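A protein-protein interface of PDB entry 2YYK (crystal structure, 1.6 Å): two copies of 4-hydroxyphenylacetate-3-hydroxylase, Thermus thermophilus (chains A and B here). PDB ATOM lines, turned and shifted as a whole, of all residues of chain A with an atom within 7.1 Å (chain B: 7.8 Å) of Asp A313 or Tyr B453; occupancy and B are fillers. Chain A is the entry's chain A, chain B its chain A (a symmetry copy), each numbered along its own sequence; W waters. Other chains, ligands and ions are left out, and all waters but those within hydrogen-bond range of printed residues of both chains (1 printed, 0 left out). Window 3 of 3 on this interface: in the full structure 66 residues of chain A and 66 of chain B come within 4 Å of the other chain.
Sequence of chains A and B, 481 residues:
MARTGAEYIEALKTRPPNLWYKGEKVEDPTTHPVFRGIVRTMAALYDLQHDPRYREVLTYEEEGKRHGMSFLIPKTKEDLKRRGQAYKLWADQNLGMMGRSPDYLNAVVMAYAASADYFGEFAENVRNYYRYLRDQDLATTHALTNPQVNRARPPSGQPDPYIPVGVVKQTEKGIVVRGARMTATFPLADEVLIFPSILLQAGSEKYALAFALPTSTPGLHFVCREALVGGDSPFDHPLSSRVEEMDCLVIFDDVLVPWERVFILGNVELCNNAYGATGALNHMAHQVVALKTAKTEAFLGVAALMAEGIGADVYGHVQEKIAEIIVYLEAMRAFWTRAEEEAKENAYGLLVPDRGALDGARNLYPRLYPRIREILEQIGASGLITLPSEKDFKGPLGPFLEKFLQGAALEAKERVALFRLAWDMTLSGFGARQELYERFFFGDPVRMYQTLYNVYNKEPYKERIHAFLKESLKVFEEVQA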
ATOM      1  N   LEU A 300      15.691   3.686 -36.119  1.00  0.00           N
ATOM      2  CA  LEU A 300      14.449   3.730 -35.356  1.00  0.00           C
ATOM      3  C   LEU A 300      14.100   2.326 -34.888  1.00  0.00           C
ATOM      4  O   LEU A 300      13.737   2.125 -33.732  1.00  0.00           O
ATOM      5  CB  LEU A 300      13.303   4.282 -36.209  1.00  0.00           C
ATOM      6  CG  LEU A 300      11.918   4.214 -35.549  1.00  0.00           C
ATOM      7  CD1 LEU A 300      11.959   4.865 -34.169  1.00  0.00           C
ATOM      8  CD2 LEU A 300      10.894   4.926 -36.433  1.00  0.00           C
ATOM      9  N   ALA A 303      16.608   1.240 -32.123  1.00  0.00           N
ATOM     10  CA  ALA A 303      16.351   1.985 -30.896  1.00  0.00           C
ATOM     11  C   ALA A 303      15.096   1.467 -30.199  1.00  0.00           C
ATOM     12  O   ALA A 303      15.087   1.273 -28.981  1.00  0.00           O
ATOM     13  CB  ALA A 303      16.196   3.478 -31.209  1.00  0.00           C
ATOM     14  N   ALA A 304      14.041   1.239 -30.976  1.00  0.00           N
ATOM     15  CA  ALA A 304      12.781   0.753 -30.421  1.00  0.00           C
ATOM     16  C   ALA A 304      12.944  -0.635 -29.809  1.00  0.00           C
ATOM     17  O   ALA A 304      12.442  -0.896 -28.715  1.00  0.00           O
ATOM     18  CB  ALA A 304      11.702   0.731 -31.504  1.00  0.00           C
ATOM     19  N   MET A 306      15.758  -1.996 -28.766  1.00  0.00           N
ATOM     20  CA  MET A 306      16.660  -1.918 -27.623  1.00  0.00           C
ATOM     21  C   MET A 306      15.890  -1.474 -26.386  1.00  0.00           C
ATOM     22  O   MET A 306      15.981  -2.097 -25.330  1.00  0.00           O
ATOM     23  CB  MET A 306      17.789  -0.921 -27.886  1.00  0.00           C
ATOM     24  CG  MET A 306      18.796  -1.369 -28.919  1.00  0.00           C
ATOM     25  SD  MET A 306      20.001  -0.064 -29.223  1.00  0.00           S
ATOM     26  CE  MET A 306      21.128  -0.344 -27.864  1.00  0.00           C
ATOM     27  N   ALA A 307      15.127  -0.395 -26.529  1.00  0.00           N
ATOM     28  CA  ALA A 307      14.350   0.146 -25.419  1.00  0.00           C
ATOM     29  C   ALA A 307      13.387  -0.893 -24.855  1.00  0.00           C
ATOM     30  O   ALA A 307      13.308  -1.081 -23.640  1.00  0.00           O
ATOM     31  CB  ALA A 307      13.578   1.389 -25.874  1.00  0.00           C
ATOM     32  N   GLU A 308      12.656  -1.570 -25.734  1.00  0.00           N
ATOM     33  CA  GLU A 308      11.710  -2.585 -25.292  1.00  0.00           C
ATOM     34  C   GLU A 308      12.435  -3.776 -24.676  1.00  0.00           C
ATOM     35  O   GLU A 308      12.027  -4.292 -23.636  1.00  0.00           O
ATOM     36  CB  GLU A 308      10.859  -3.057 -26.468  1.00  0.00           C
ATOM     37  CG  GLU A 308      10.017  -1.961 -27.090  1.00  0.00           C
ATOM     38  CD  GLU A 308       9.198  -2.453 -28.265  1.00  0.00           C
ATOM     39  OE1 GLU A 308       8.495  -1.625 -28.883  1.00  0.00           O
ATOM     40  OE2 GLU A 308       9.258  -3.664 -28.571  1.00  0.00           O
ATOM     41  N   GLY A 309      13.522  -4.195 -25.315  1.00  0.00           N
ATOM     42  CA  GLY A 309      14.282  -5.336 -24.830  1.00  0.00           C
ATOM     43  C   GLY A 309      14.844  -5.219 -23.426  1.00  0.00           C
ATOM     44  O   GLY A 309      14.976  -6.229 -22.728  1.00  0.00           O
ATOM     45  N   ILE A 310      15.191  -4.004 -23.009  1.00  0.00           N
ATOM     46  CA  ILE A 310      15.745  -3.784 -21.676  1.00  0.00           C
ATOM     47  C   ILE A 310      14.756  -3.063 -20.760  1.00  0.00           C
ATOM     48  O   ILE A 310      15.110  -2.642 -19.657  1.00  0.00           O
ATOM     49  CB  ILE A 310      17.060  -2.969 -21.740  1.00  0.00           C
ATOM     50  CG1 ILE A 310      16.785  -1.575 -22.309  1.00  0.00           C
ATOM     51  CG2 ILE A 310      18.084  -3.703 -22.595  1.00  0.00           C
ATOM     52  CD1 ILE A 310      18.011  -0.687 -22.371  1.00  0.00           C
ATOM     53  N   GLY A 311      13.517  -2.922 -21.227  1.00  0.00           N
ATOM     54  CA  GLY A 311      12.487  -2.272 -20.433  1.00  0.00           C
ATOM     55  C   GLY A 311      12.703  -0.787 -20.212  1.00  0.00           C
ATOM     56  O   GLY A 311      12.102  -0.189 -19.317  1.00  0.00           O
ATOM     57  N   ALA A 312      13.561  -0.189 -21.029  1.00  0.00           N
ATOM     58  CA  ALA A 312      13.862   1.231 -20.917  1.00  0.00           C
ATOM     59  C   ALA A 312      12.771   2.081 -21.552  1.00  0.00           C
ATOM     60  O   ALA A 312      12.753   3.304 -21.383  1.00  0.00           O
ATOM     61  CB  ALA A 312      15.205   1.529 -21.578  1.00  0.00           C
ATOM     62  N   ASP A 313      11.862   1.435 -22.274  1.00  0.00           N
ATOM     63  CA  ASP A 313      10.778   2.148 -22.939  1.00  0.00           C
ATOM     64  C   ASP A 313       9.772   2.762 -21.968  1.00  0.00           C
ATOM     65  O   ASP A 313       8.899   3.526 -22.377  1.00  0.00           O
ATOM     66  CB  ASP A 313      10.045   1.226 -23.919  1.00  0.00           C
ATOM     67  CG  ASP A 313       9.493  -0.023 -23.254  1.00  0.00           C
ATOM     68  OD1 ASP A 313       8.562  -0.630 -23.822  1.00  0.00           O
ATOM     69  OD2 ASP A 313       9.993  -0.410 -22.176  1.00  0.00           O
ATOM     70  N   VAL A 314       9.893   2.429 -20.686  1.00  0.00           N
ATOM     71  CA  VAL A 314       8.984   2.971 -19.680  1.00  0.00           C
ATOM     72  C   VAL A 314       9.481   4.331 -19.204  1.00  0.00           C
ATOM     73  O   VAL A 314       8.772   5.055 -18.505  1.00  0.00           O
ATOM     74  CB  VAL A 314       8.860   2.027 -18.457  1.00  0.00           C
ATOM     75  CG1 VAL A 314       8.379   0.658 -18.910  1.00  0.00           C
ATOM     76  CG2 VAL A 314      10.192   1.919 -17.736  1.00  0.00           C
ATOM     77  N   TYR A 315      10.707   4.669 -19.592  1.00  0.00           N
ATOM     78  CA  TYR A 315      11.313   5.937 -19.214  1.00  0.00           C
ATOM     79  C   TYR A 315      10.957   7.035 -20.209  1.00  0.00           C
ATOM     80  O   TYR A 315      11.164   6.885 -21.417  1.00  0.00           O
ATOM     81  CB  TYR A 315      12.835   5.800 -19.141  1.00  0.00           C
ATOM     82  CG  TYR A 315      13.328   4.895 -18.034  1.00  0.00           C
ATOM     83  CD1 TYR A 315      13.044   5.179 -16.697  1.00  0.00           C
ATOM     84  CD2 TYR A 315      14.090   3.763 -18.317  1.00  0.00           C
ATOM     85  CE1 TYR A 315      13.508   4.359 -15.672  1.00  0.00           C
ATOM     86  CE2 TYR A 315      14.560   2.935 -17.300  1.00  0.00           C
ATOM     87  CZ  TYR A 315      14.265   3.240 -15.980  1.00  0.00           C
ATOM     88  OH  TYR A 315      14.728   2.429 -14.969  1.00  0.00           O
ATOM     89  N   GLY A 316      10.429   8.140 -19.692  1.00  0.00           N
ATOM     90  CA  GLY A 316      10.060   9.255 -20.545  1.00  0.00           C
ATOM     91  C   GLY A 316      11.226   9.720 -21.394  1.00  0.00           C
ATOM     92  O   GLY A 316      11.059  10.011 -22.582  1.00  0.00           O
ATOM     93  N   VAL A 318      13.723   8.066 -22.598  1.00  0.00           N
ATOM     94  CA  VAL A 318      13.976   7.176 -23.722  1.00  0.00           C
ATOM     95  C   VAL A 318      12.905   7.328 -24.794  1.00  0.00           C
ATOM     96  O   VAL A 318      13.219   7.325 -25.984  1.00  0.00           O
ATOM     97  CB  VAL A 318      14.063   5.703 -23.260  1.00  0.00           C
ATOM     98  CG1 VAL A 318      14.234   4.781 -24.457  1.00  0.00           C
ATOM     99  CG2 VAL A 318      15.236   5.540 -22.306  1.00  0.00           C
ATOM    100  N   GLN A 319      11.651   7.470 -24.376  1.00  0.00           N
ATOM    101  CA  GLN A 319      10.560   7.641 -25.329  1.00  0.00           C
ATOM    102  C   GLN A 319      10.808   8.910 -26.133  1.00  0.00           C
ATOM    103  O   GLN A 319      10.583   8.942 -27.341  1.00  0.00           O
ATOM    104  CB  GLN A 319       9.213   7.759 -24.606  1.00  0.00           C
ATOM    105  CG  GLN A 319       8.870   6.564 -23.730  1.00  0.00           C
ATOM    106  CD  GLN A 319       7.497   6.682 -23.094  1.00  0.00           C
ATOM    107  OE1 GLN A 319       6.925   7.768 -23.024  1.00  0.00           O
ATOM    108  NE2 GLN A 319       6.967   5.563 -22.617  1.00  0.00           N
ATOM    109  N   GLU A 320      11.264   9.956 -25.450  1.00  0.00           N
ATOM    110  CA  GLU A 320      11.537  11.235 -26.095  1.00  0.00           C
ATOM    111  C   GLU A 320      12.637  11.123 -27.143  1.00  0.00           C
ATOM    112  O   GLU A 320      12.545  11.729 -28.210  1.00  0.00           O
ATOM    113  CB  GLU A 320      11.920  12.279 -25.046  1.00  0.00           C
ATOM    114  CG  GLU A 320      10.825  12.489 -24.018  1.00  0.00           C
ATOM    115  CD  GLU A 320      11.251  13.376 -22.869  1.00  0.00           C
ATOM    116  OE1 GLU A 320      10.715  13.188 -21.759  1.00  0.00           O
ATOM    117  OE2 GLU A 320      12.107  14.263 -23.076  1.00  0.00           O
ATOM    118  N   LYS A 321      13.680  10.353 -26.838  1.00  0.00           N
ATOM    119  CA  LYS A 321      14.779  10.177 -27.785  1.00  0.00           C
ATOM    120  C   LYS A 321      14.303   9.415 -29.023  1.00  0.00           C
ATOM    121  O   LYS A 321      14.706   9.723 -30.145  1.00  0.00           O
ATOM    122  CB  LYS A 321      15.940   9.417 -27.137  1.00  0.00           C
ATOM    123  CG  LYS A 321      16.599  10.155 -25.985  1.00  0.00           C
ATOM    124  CD  LYS A 321      17.698   9.303 -25.353  1.00  0.00           C
ATOM    125  CE  LYS A 321      18.199   9.914 -24.052  1.00  0.00           C
ATOM    126  NZ  LYS A 321      18.748  11.276 -24.260  1.00  0.00           N
ATOM    127  N   ILE A 322      13.444   8.422 -28.824  1.00  0.00           N
ATOM    128  CA  ILE A 322      12.936   7.657 -29.955  1.00  0.00           C
ATOM    129  C   ILE A 322      12.007   8.546 -30.785  1.00  0.00           C
ATOM    130  O   ILE A 322      12.010   8.481 -32.017  1.00  0.00           O
ATOM    131  CB  ILE A 322      12.217   6.377 -29.473  1.00  0.00           C
ATOM    132  CG1 ILE A 322      13.245   5.448 -28.819  1.00  0.00           C
ATOM    133  CG2 ILE A 322      11.548   5.666 -30.639  1.00  0.00           C
ATOM    134  CD1 ILE A 322      12.663   4.183 -28.213  1.00  0.00           C
ATOM    135  N   ALA A 323      11.226   9.386 -30.114  1.00  0.00           N
ATOM    136  CA  ALA A 323      10.337  10.310 -30.813  1.00  0.00           C
ATOM    137  C   ALA A 323      11.170  11.300 -31.636  1.00  0.00           C
ATOM    138  O   ALA A 323      10.735  11.764 -32.695  1.00  0.00           O
ATOM    139  CB  ALA A 323       9.461  11.058 -29.807  1.00  0.00           C
ATOM    140  N   ILE A 326      11.989   9.731 -34.730  1.00  0.00           N
ATOM    141  CA  ILE A 326      10.785   9.739 -35.560  1.00  0.00           C
ATOM    142  C   ILE A 326      10.618  11.089 -36.266  1.00  0.00           C
ATOM    143  O   ILE A 326      10.263  11.135 -37.443  1.00  0.00           O
ATOM    144  CB  ILE A 326       9.527   9.423 -34.712  1.00  0.00           C
ATOM    145  CG1 ILE A 326       9.569   7.956 -34.272  1.00  0.00           C
ATOM    146  CG2 ILE A 326       8.258   9.700 -35.521  1.00  0.00           C
ATOM    147  CD1 ILE A 326       8.554   7.600 -33.187  1.00  0.00           C
ATOM    148  N   ASP B 359       3.147  16.024 -37.365  1.00  0.00           N
ATOM    149  CA  ASP B 359       3.749  15.767 -36.056  1.00  0.00           C
ATOM    150  C   ASP B 359       5.231  16.128 -36.160  1.00  0.00           C
ATOM    151  O   ASP B 359       5.823  16.647 -35.216  1.00  0.00           O
ATOM    152  CB  ASP B 359       3.592  14.292 -35.650  1.00  0.00           C
ATOM    153  CG  ASP B 359       2.279  14.019 -34.929  1.00  0.00           C
ATOM    154  OD1 ASP B 359       1.958  12.835 -34.696  1.00  0.00           O
ATOM    155  OD2 ASP B 359       1.571  14.985 -34.580  1.00  0.00           O
ATOM    156  N   ASN B 363       6.678  19.272 -33.899  1.00  0.00           N
ATOM    157  CA  ASN B 363       7.612  18.860 -32.858  1.00  0.00           C
ATOM    158  C   ASN B 363       9.028  19.326 -33.164  1.00  0.00           C
ATOM    159  O   ASN B 363       9.891  19.338 -32.282  1.00  0.00           O
ATOM    160  CB  ASN B 363       7.557  17.346 -32.654  1.00  0.00           C
ATOM    161  CG  ASN B 363       6.390  16.941 -31.785  1.00  0.00           C
ATOM    162  OD1 ASN B 363       6.345  17.291 -30.605  1.00  0.00           O
ATOM    163  ND2 ASN B 363       5.428  16.225 -32.361  1.00  0.00           N
ATOM    164  N   ARG B 447       5.719  16.258 -23.132  1.00  0.00           N
ATOM    165  CA  ARG B 447       4.476  15.513 -23.305  1.00  0.00           C
ATOM    166  C   ARG B 447       4.223  15.244 -24.789  1.00  0.00           C
ATOM    167  O   ARG B 447       3.754  14.172 -25.166  1.00  0.00           O
ATOM    168  CB  ARG B 447       3.308  16.304 -22.706  1.00  0.00           C
ATOM    169  CG  ARG B 447       1.992  15.540 -22.589  1.00  0.00           C
ATOM    170  CD  ARG B 447       1.352  15.280 -23.943  1.00  0.00           C
ATOM    171  NE  ARG B 447       1.129  16.515 -24.688  1.00  0.00           N
ATOM    172  CZ  ARG B 447       0.644  16.562 -25.925  1.00  0.00           C
ATOM    173  NH1 ARG B 447       0.330  15.441 -26.558  1.00  0.00           N
ATOM    174  NH2 ARG B 447       0.475  17.730 -26.529  1.00  0.00           N
ATOM    175  N   MET B 448       4.525  16.228 -25.630  1.00  0.00           N
ATOM    176  CA  MET B 448       4.322  16.070 -27.063  1.00  0.00           C
ATOM    177  C   MET B 448       5.179  14.947 -27.639  1.00  0.00           C
ATOM    178  O   MET B 448       4.715  14.166 -28.468  1.00  0.00           O
ATOM    179  CB  MET B 448       4.623  17.384 -27.786  1.00  0.00           C
ATOM    180  CG  MET B 448       3.587  18.457 -27.529  1.00  0.00           C
ATOM    181  SD  MET B 448       3.940  20.003 -28.383  1.00  0.00           S
ATOM    182  CE  MET B 448       3.665  19.502 -30.099  1.00  0.00           C
ATOM    183  N   TYR B 449       6.427  14.860 -27.191  1.00  0.00           N
ATOM    184  CA  TYR B 449       7.310  13.815 -27.689  1.00  0.00           C
ATOM    185  C   TYR B 449       6.880  12.445 -27.164  1.00  0.00           C
ATOM    186  O   TYR B 449       6.966  11.445 -27.878  1.00  0.00           O
ATOM    187  CB  TYR B 449       8.769  14.127 -27.322  1.00  0.00           C
ATOM    188  CG  TYR B 449       9.475  14.973 -28.369  1.00  0.00           C
ATOM    189  CD1 TYR B 449       9.015  16.256 -28.689  1.00  0.00           C
ATOM    190  CD2 TYR B 449      10.580  14.482 -29.065  1.00  0.00           C
ATOM    191  CE1 TYR B 449       9.636  17.022 -29.681  1.00  0.00           C
ATOM    192  CE2 TYR B 449      11.207  15.238 -30.059  1.00  0.00           C
ATOM    193  CZ  TYR B 449      10.730  16.505 -30.363  1.00  0.00           C
ATOM    194  OH  TYR B 449      11.343  17.244 -31.353  1.00  0.00           O
ATOM    195  N   GLN B 450       6.407  12.391 -25.924  1.00  0.00           N
ATOM    196  CA  GLN B 450       5.945  11.122 -25.374  1.00  0.00           C
ATOM    197  C   GLN B 450       4.674  10.689 -26.122  1.00  0.00           C
ATOM    198  O   GLN B 450       4.463   9.503 -26.385  1.00  0.00           O
ATOM    199  CB  GLN B 450       5.696  11.263 -23.866  1.00  0.00           C
ATOM    200  CG  GLN B 450       7.000  11.292 -23.062  1.00  0.00           C
ATOM    201  CD  GLN B 450       6.792  11.546 -21.580  1.00  0.00           C
ATOM    202  OE1 GLN B 450       5.756  11.198 -21.019  1.00  0.00           O
ATOM    203  NE2 GLN B 450       7.791  12.143 -20.934  1.00  0.00           N
ATOM    204  N   THR B 451       3.839  11.656 -26.492  1.00  0.00           N
ATOM    205  CA  THR B 451       2.622  11.351 -27.236  1.00  0.00           C
ATOM    206  C   THR B 451       2.999  10.808 -28.617  1.00  0.00           C
ATOM    207  O   THR B 451       2.415   9.834 -29.090  1.00  0.00           O
ATOM    208  CB  THR B 451       1.737  12.603 -27.394  1.00  0.00           C
ATOM    209  OG1 THR B 451       1.169  12.940 -26.121  1.00  0.00           O
ATOM    210  CG2 THR B 451       0.618  12.353 -28.396  1.00  0.00           C
ATOM    211  N   LEU B 452       3.984  11.430 -29.257  1.00  0.00           N
ATOM    212  CA  LEU B 452       4.423  10.974 -30.571  1.00  0.00           C
ATOM    213  C   LEU B 452       4.950   9.544 -30.486  1.00  0.00           C
ATOM    214  O   LEU B 452       4.658   8.708 -31.344  1.00  0.00           O
ATOM    215  CB  LEU B 452       5.513  11.898 -31.126  1.00  0.00           C
ATOM    216  CG  LEU B 452       6.126  11.474 -32.465  1.00  0.00           C
ATOM    217  CD1 LEU B 452       5.025  11.286 -33.507  1.00  0.00           C
ATOM    218  CD2 LEU B 452       7.123  12.538 -32.931  1.00  0.00           C
ATOM    219  N   TYR B 453       5.730   9.262 -29.448  1.00  0.00           N
ATOM    220  CA  TYR B 453       6.276   7.925 -29.274  1.00  0.00           C
ATOM    221  C   TYR B 453       5.168   6.884 -29.161  1.00  0.00           C
ATOM    222  O   TYR B 453       5.226   5.825 -29.794  1.00  0.00           O
ATOM    223  CB  TYR B 453       7.153   7.858 -28.016  1.00  0.00           C
ATOM    224  CG  TYR B 453       7.543   6.443 -27.646  1.00  0.00           C
ATOM    225  CD1 TYR B 453       6.759   5.686 -26.776  1.00  0.00           C
ATOM    226  CD2 TYR B 453       8.660   5.839 -28.219  1.00  0.00           C
ATOM    227  CE1 TYR B 453       7.076   4.358 -26.491  1.00  0.00           C
ATOM    228  CE2 TYR B 453       8.986   4.512 -27.941  1.00  0.00           C
ATOM    229  CZ  TYR B 453       8.191   3.780 -27.080  1.00  0.00           C
ATOM    230  OH  TYR B 453       8.508   2.466 -26.815  1.00  0.00           O
ATOM    231  N   ASN B 454       4.154   7.190 -28.364  1.00  0.00           N
ATOM    232  CA  ASN B 454       3.060   6.250 -28.151  1.00  0.00           C
ATOM    233  C   ASN B 454       2.123   6.019 -29.332  1.00  0.00           C
ATOM    234  O   ASN B 454       1.650   4.901 -29.536  1.00  0.00           O
ATOM    235  CB  ASN B 454       2.256   6.665 -26.919  1.00  0.00           C
ATOM    236  CG  ASN B 454       3.034   6.466 -25.630  1.00  0.00           C
ATOM    237  OD1 ASN B 454       3.501   5.362 -25.339  1.00  0.00           O
ATOM    238  ND2 ASN B 454       3.177   7.531 -24.853  1.00  0.00           N
ATOM    239  N   VAL B 455       1.866   7.057 -30.123  1.00  0.00           N
ATOM    240  CA  VAL B 455       0.958   6.917 -31.258  1.00  0.00           C
ATOM    241  C   VAL B 455       1.601   6.393 -32.541  1.00  0.00           C
ATOM    242  O   VAL B 455       0.924   5.809 -33.386  1.00  0.00           O
ATOM    243  CB  VAL B 455       0.258   8.263 -31.578  1.00  0.00           C
ATOM    244  CG1 VAL B 455       1.272   9.273 -32.089  1.00  0.00           C
ATOM    245  CG2 VAL B 455      -0.836   8.050 -32.607  1.00  0.00           C
ATOM    246  N   TYR B 456       2.909   6.576 -32.682  1.00  0.00           N
ATOM    247  CA  TYR B 456       3.601   6.151 -33.895  1.00  0.00           C
ATOM    248  C   TYR B 456       3.723   4.640 -34.066  1.00  0.00           C
ATOM    249  O   TYR B 456       4.089   3.925 -33.131  1.00  0.00           O
ATOM    250  CB  TYR B 456       5.002   6.769 -33.935  1.00  0.00           C
ATOM    251  CG  TYR B 456       5.561   6.949 -35.329  1.00  0.00           C
ATOM    252  CD1 TYR B 456       5.141   8.004 -36.140  1.00  0.00           C
ATOM    253  CD2 TYR B 456       6.532   6.084 -35.827  1.00  0.00           C
ATOM    254  CE1 TYR B 456       5.684   8.198 -37.413  1.00  0.00           C
ATOM    255  CE2 TYR B 456       7.079   6.262 -37.095  1.00  0.00           C
ATOM    256  CZ  TYR B 456       6.654   7.324 -37.881  1.00  0.00           C
ATOM    257  OH  TYR B 456       7.218   7.518 -39.118  1.00  0.00           O
ATOM    258  N   ASN B 457       3.426   4.158 -35.271  1.00  0.00           N
ATOM    259  CA  ASN B 457       3.542   2.733 -35.555  1.00  0.00           C
ATOM    260  C   ASN B 457       5.006   2.426 -35.838  1.00  0.00           C
ATOM    261  O   ASN B 457       5.516   2.706 -36.924  1.00  0.00           O
ATOM    262  CB  ASN B 457       2.689   2.342 -36.763  1.00  0.00           C
ATOM    263  CG  ASN B 457       2.840   0.881 -37.126  1.00  0.00           C
ATOM    264  OD1 ASN B 457       3.278   0.073 -36.305  1.00  0.00           O
ATOM    265  ND2 ASN B 457       2.469   0.529 -38.353  1.00  0.00           N
ATOM    266  N   LYS B 458       5.677   1.854 -34.847  1.00  0.00           N
ATOM    267  CA  LYS B 458       7.088   1.517 -34.970  1.00  0.00           C
ATOM    268  C   LYS B 458       7.317   0.079 -35.431  1.00  0.00           C
ATOM    269  O   LYS B 458       8.454  -0.332 -35.647  1.00  0.00           O
ATOM    270  CB  LYS B 458       7.774   1.739 -33.621  1.00  0.00           C
ATOM    271  CG  LYS B 458       7.623   3.159 -33.097  1.00  0.00           C
ATOM    272  CD  LYS B 458       8.036   3.287 -31.637  1.00  0.00           C
ATOM    273  CE  LYS B 458       7.039   2.614 -30.697  1.00  0.00           C
ATOM    274  NZ  LYS B 458       5.691   3.261 -30.728  1.00  0.00           N
ATOM    275  N   LYS B 462      10.797  -2.317 -36.538  1.00  0.00           N
ATOM    276  CA  LYS B 462      11.181  -3.362 -35.603  1.00  0.00           C
ATOM    277  C   LYS B 462      11.207  -4.692 -36.351  1.00  0.00           C
ATOM    278  O   LYS B 462      12.097  -5.518 -36.137  1.00  0.00           O
ATOM    279  CB  LYS B 462      10.181  -3.419 -34.445  1.00  0.00           C
ATOM    280  CG  LYS B 462      10.232  -2.190 -33.547  1.00  0.00           C
ATOM    281  CD  LYS B 462       9.009  -2.087 -32.641  1.00  0.00           C
ATOM    282  CE  LYS B 462       8.914  -3.253 -31.675  1.00  0.00           C
ATOM    283  NZ  LYS B 462       7.709  -3.127 -30.809  1.00  0.00           N
HETATM  284  O   HOH W   1       6.783   0.995 -25.449  1.00  0.00           O
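Along chain A the printed residues that touch a printed residue of chain B span positions 304 to 326. Among the printed residues, Asp or Glu carboxylates within 4 Å of a Lys or Arg side-chain nitrogen of the other chain: Glu A308 with Lys B462 (2.6 Å).
Water W1 bridges the side-chain hydroxyl (OH) of Tyr B453 (2.6 Å) and the side-chain carboxylate (OD1) of Asp A313 (2.9 Å).
The side-chain carboxylate (OE1) of Glu A308 is in salt-bridge range of the side-chain amino group (NZ) of Lys B462, 2.6 Å away. The side-chain carboxylate of Glu A320 lies within hydrogen-bond range of the side-chain amide nitrogen of Gln B450.
O of Ala A307 is in hydrogen-bond range of N of Asp A313 (3.2 Å). The backbone carbonyl oxygen (O) of Asp A313 is in hydrogen-bond range of the side-chain amide nitrogen (NE2) of Gln A319, at 2.8 Å. The side-chain hydroxyl (OH) of Tyr B449 is in hydrogen-bond range of the backbone carbonyl oxygen (O) of Asn B363 (2.7 Å). The side-chain amide nitrogen (ND2) of Asn B454 is in hydrogen-bond range of the backbone carbonyl oxygen (O) of Gln B450, 2.8 Å away. The side-chain amino group of Lys B458 is in hydrogen-bond range of the backbone carbonyl oxygen of Tyr B453, at 2.8 Å. The backbone carbonyl oxygen of Tyr B456 is in hydrogen-bond range of the side-chain amino group of Lys B458 (3.0 Å).
Of the printed residues of chain B, Glu A308 touches Lys B462 (2.6 Å). Ala A312 touches none of the printed residues of chain B. Asp A313 touches one residue of chain B. Of the printed residues of chain B, Glu A320 touches Tyr B449 (3.5 Å) and Gln B450 (3.2 Å). Printed residues of chain B within 4 Å of Ile A326: Tyr B456. Printed residues of chain A within 4 Å of Gln B450: Gly A316 (3.7 Å), Gln A319 (3.5 Å) and Glu A320 (3.2 Å). Of the printed residues of chain A, Tyr B453 touches Asp A313 (3.5 Å), Gln A319 (3.7 Å) and Ile A322 (3.7 Å). Printed residues of chain A within 4 Å of Lys B462: Ala A304 and Glu A308. The nearest residue of chain B that does not touch Asp A313 is Asn B454 (6.4 Å). The nearest residue of chain A that does not touch Tyr B453 is Ala A323 (4.2 Å).
No position is printed for both chains. Of the 12 pairs that touch across the chains among the printed residues, none has its exchanged pair printed and touching as well.
Ala A304 touches Lys B462 (CB to CG, 3.9 Å). Asp A313 touches Tyr B453. NE2 of Gln B450 touches CA of Gly A316, at 3.7 Å. Gln B450 touches Gln A319. O of Gln A319 touches CB of Tyr B453 (3.7 Å). Glu A320 touches Tyr B449 (O to CD2, 3.5 Å). Ile A322 touches Tyr B453. CB of Ala A323 touches O of Tyr B449 (3.2 Å). CD2 of Leu B452 touches O of Ala A323 (3.7 Å). CE1 of Tyr B456 touches CG2 of Ile A326, at 3.5 Å.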
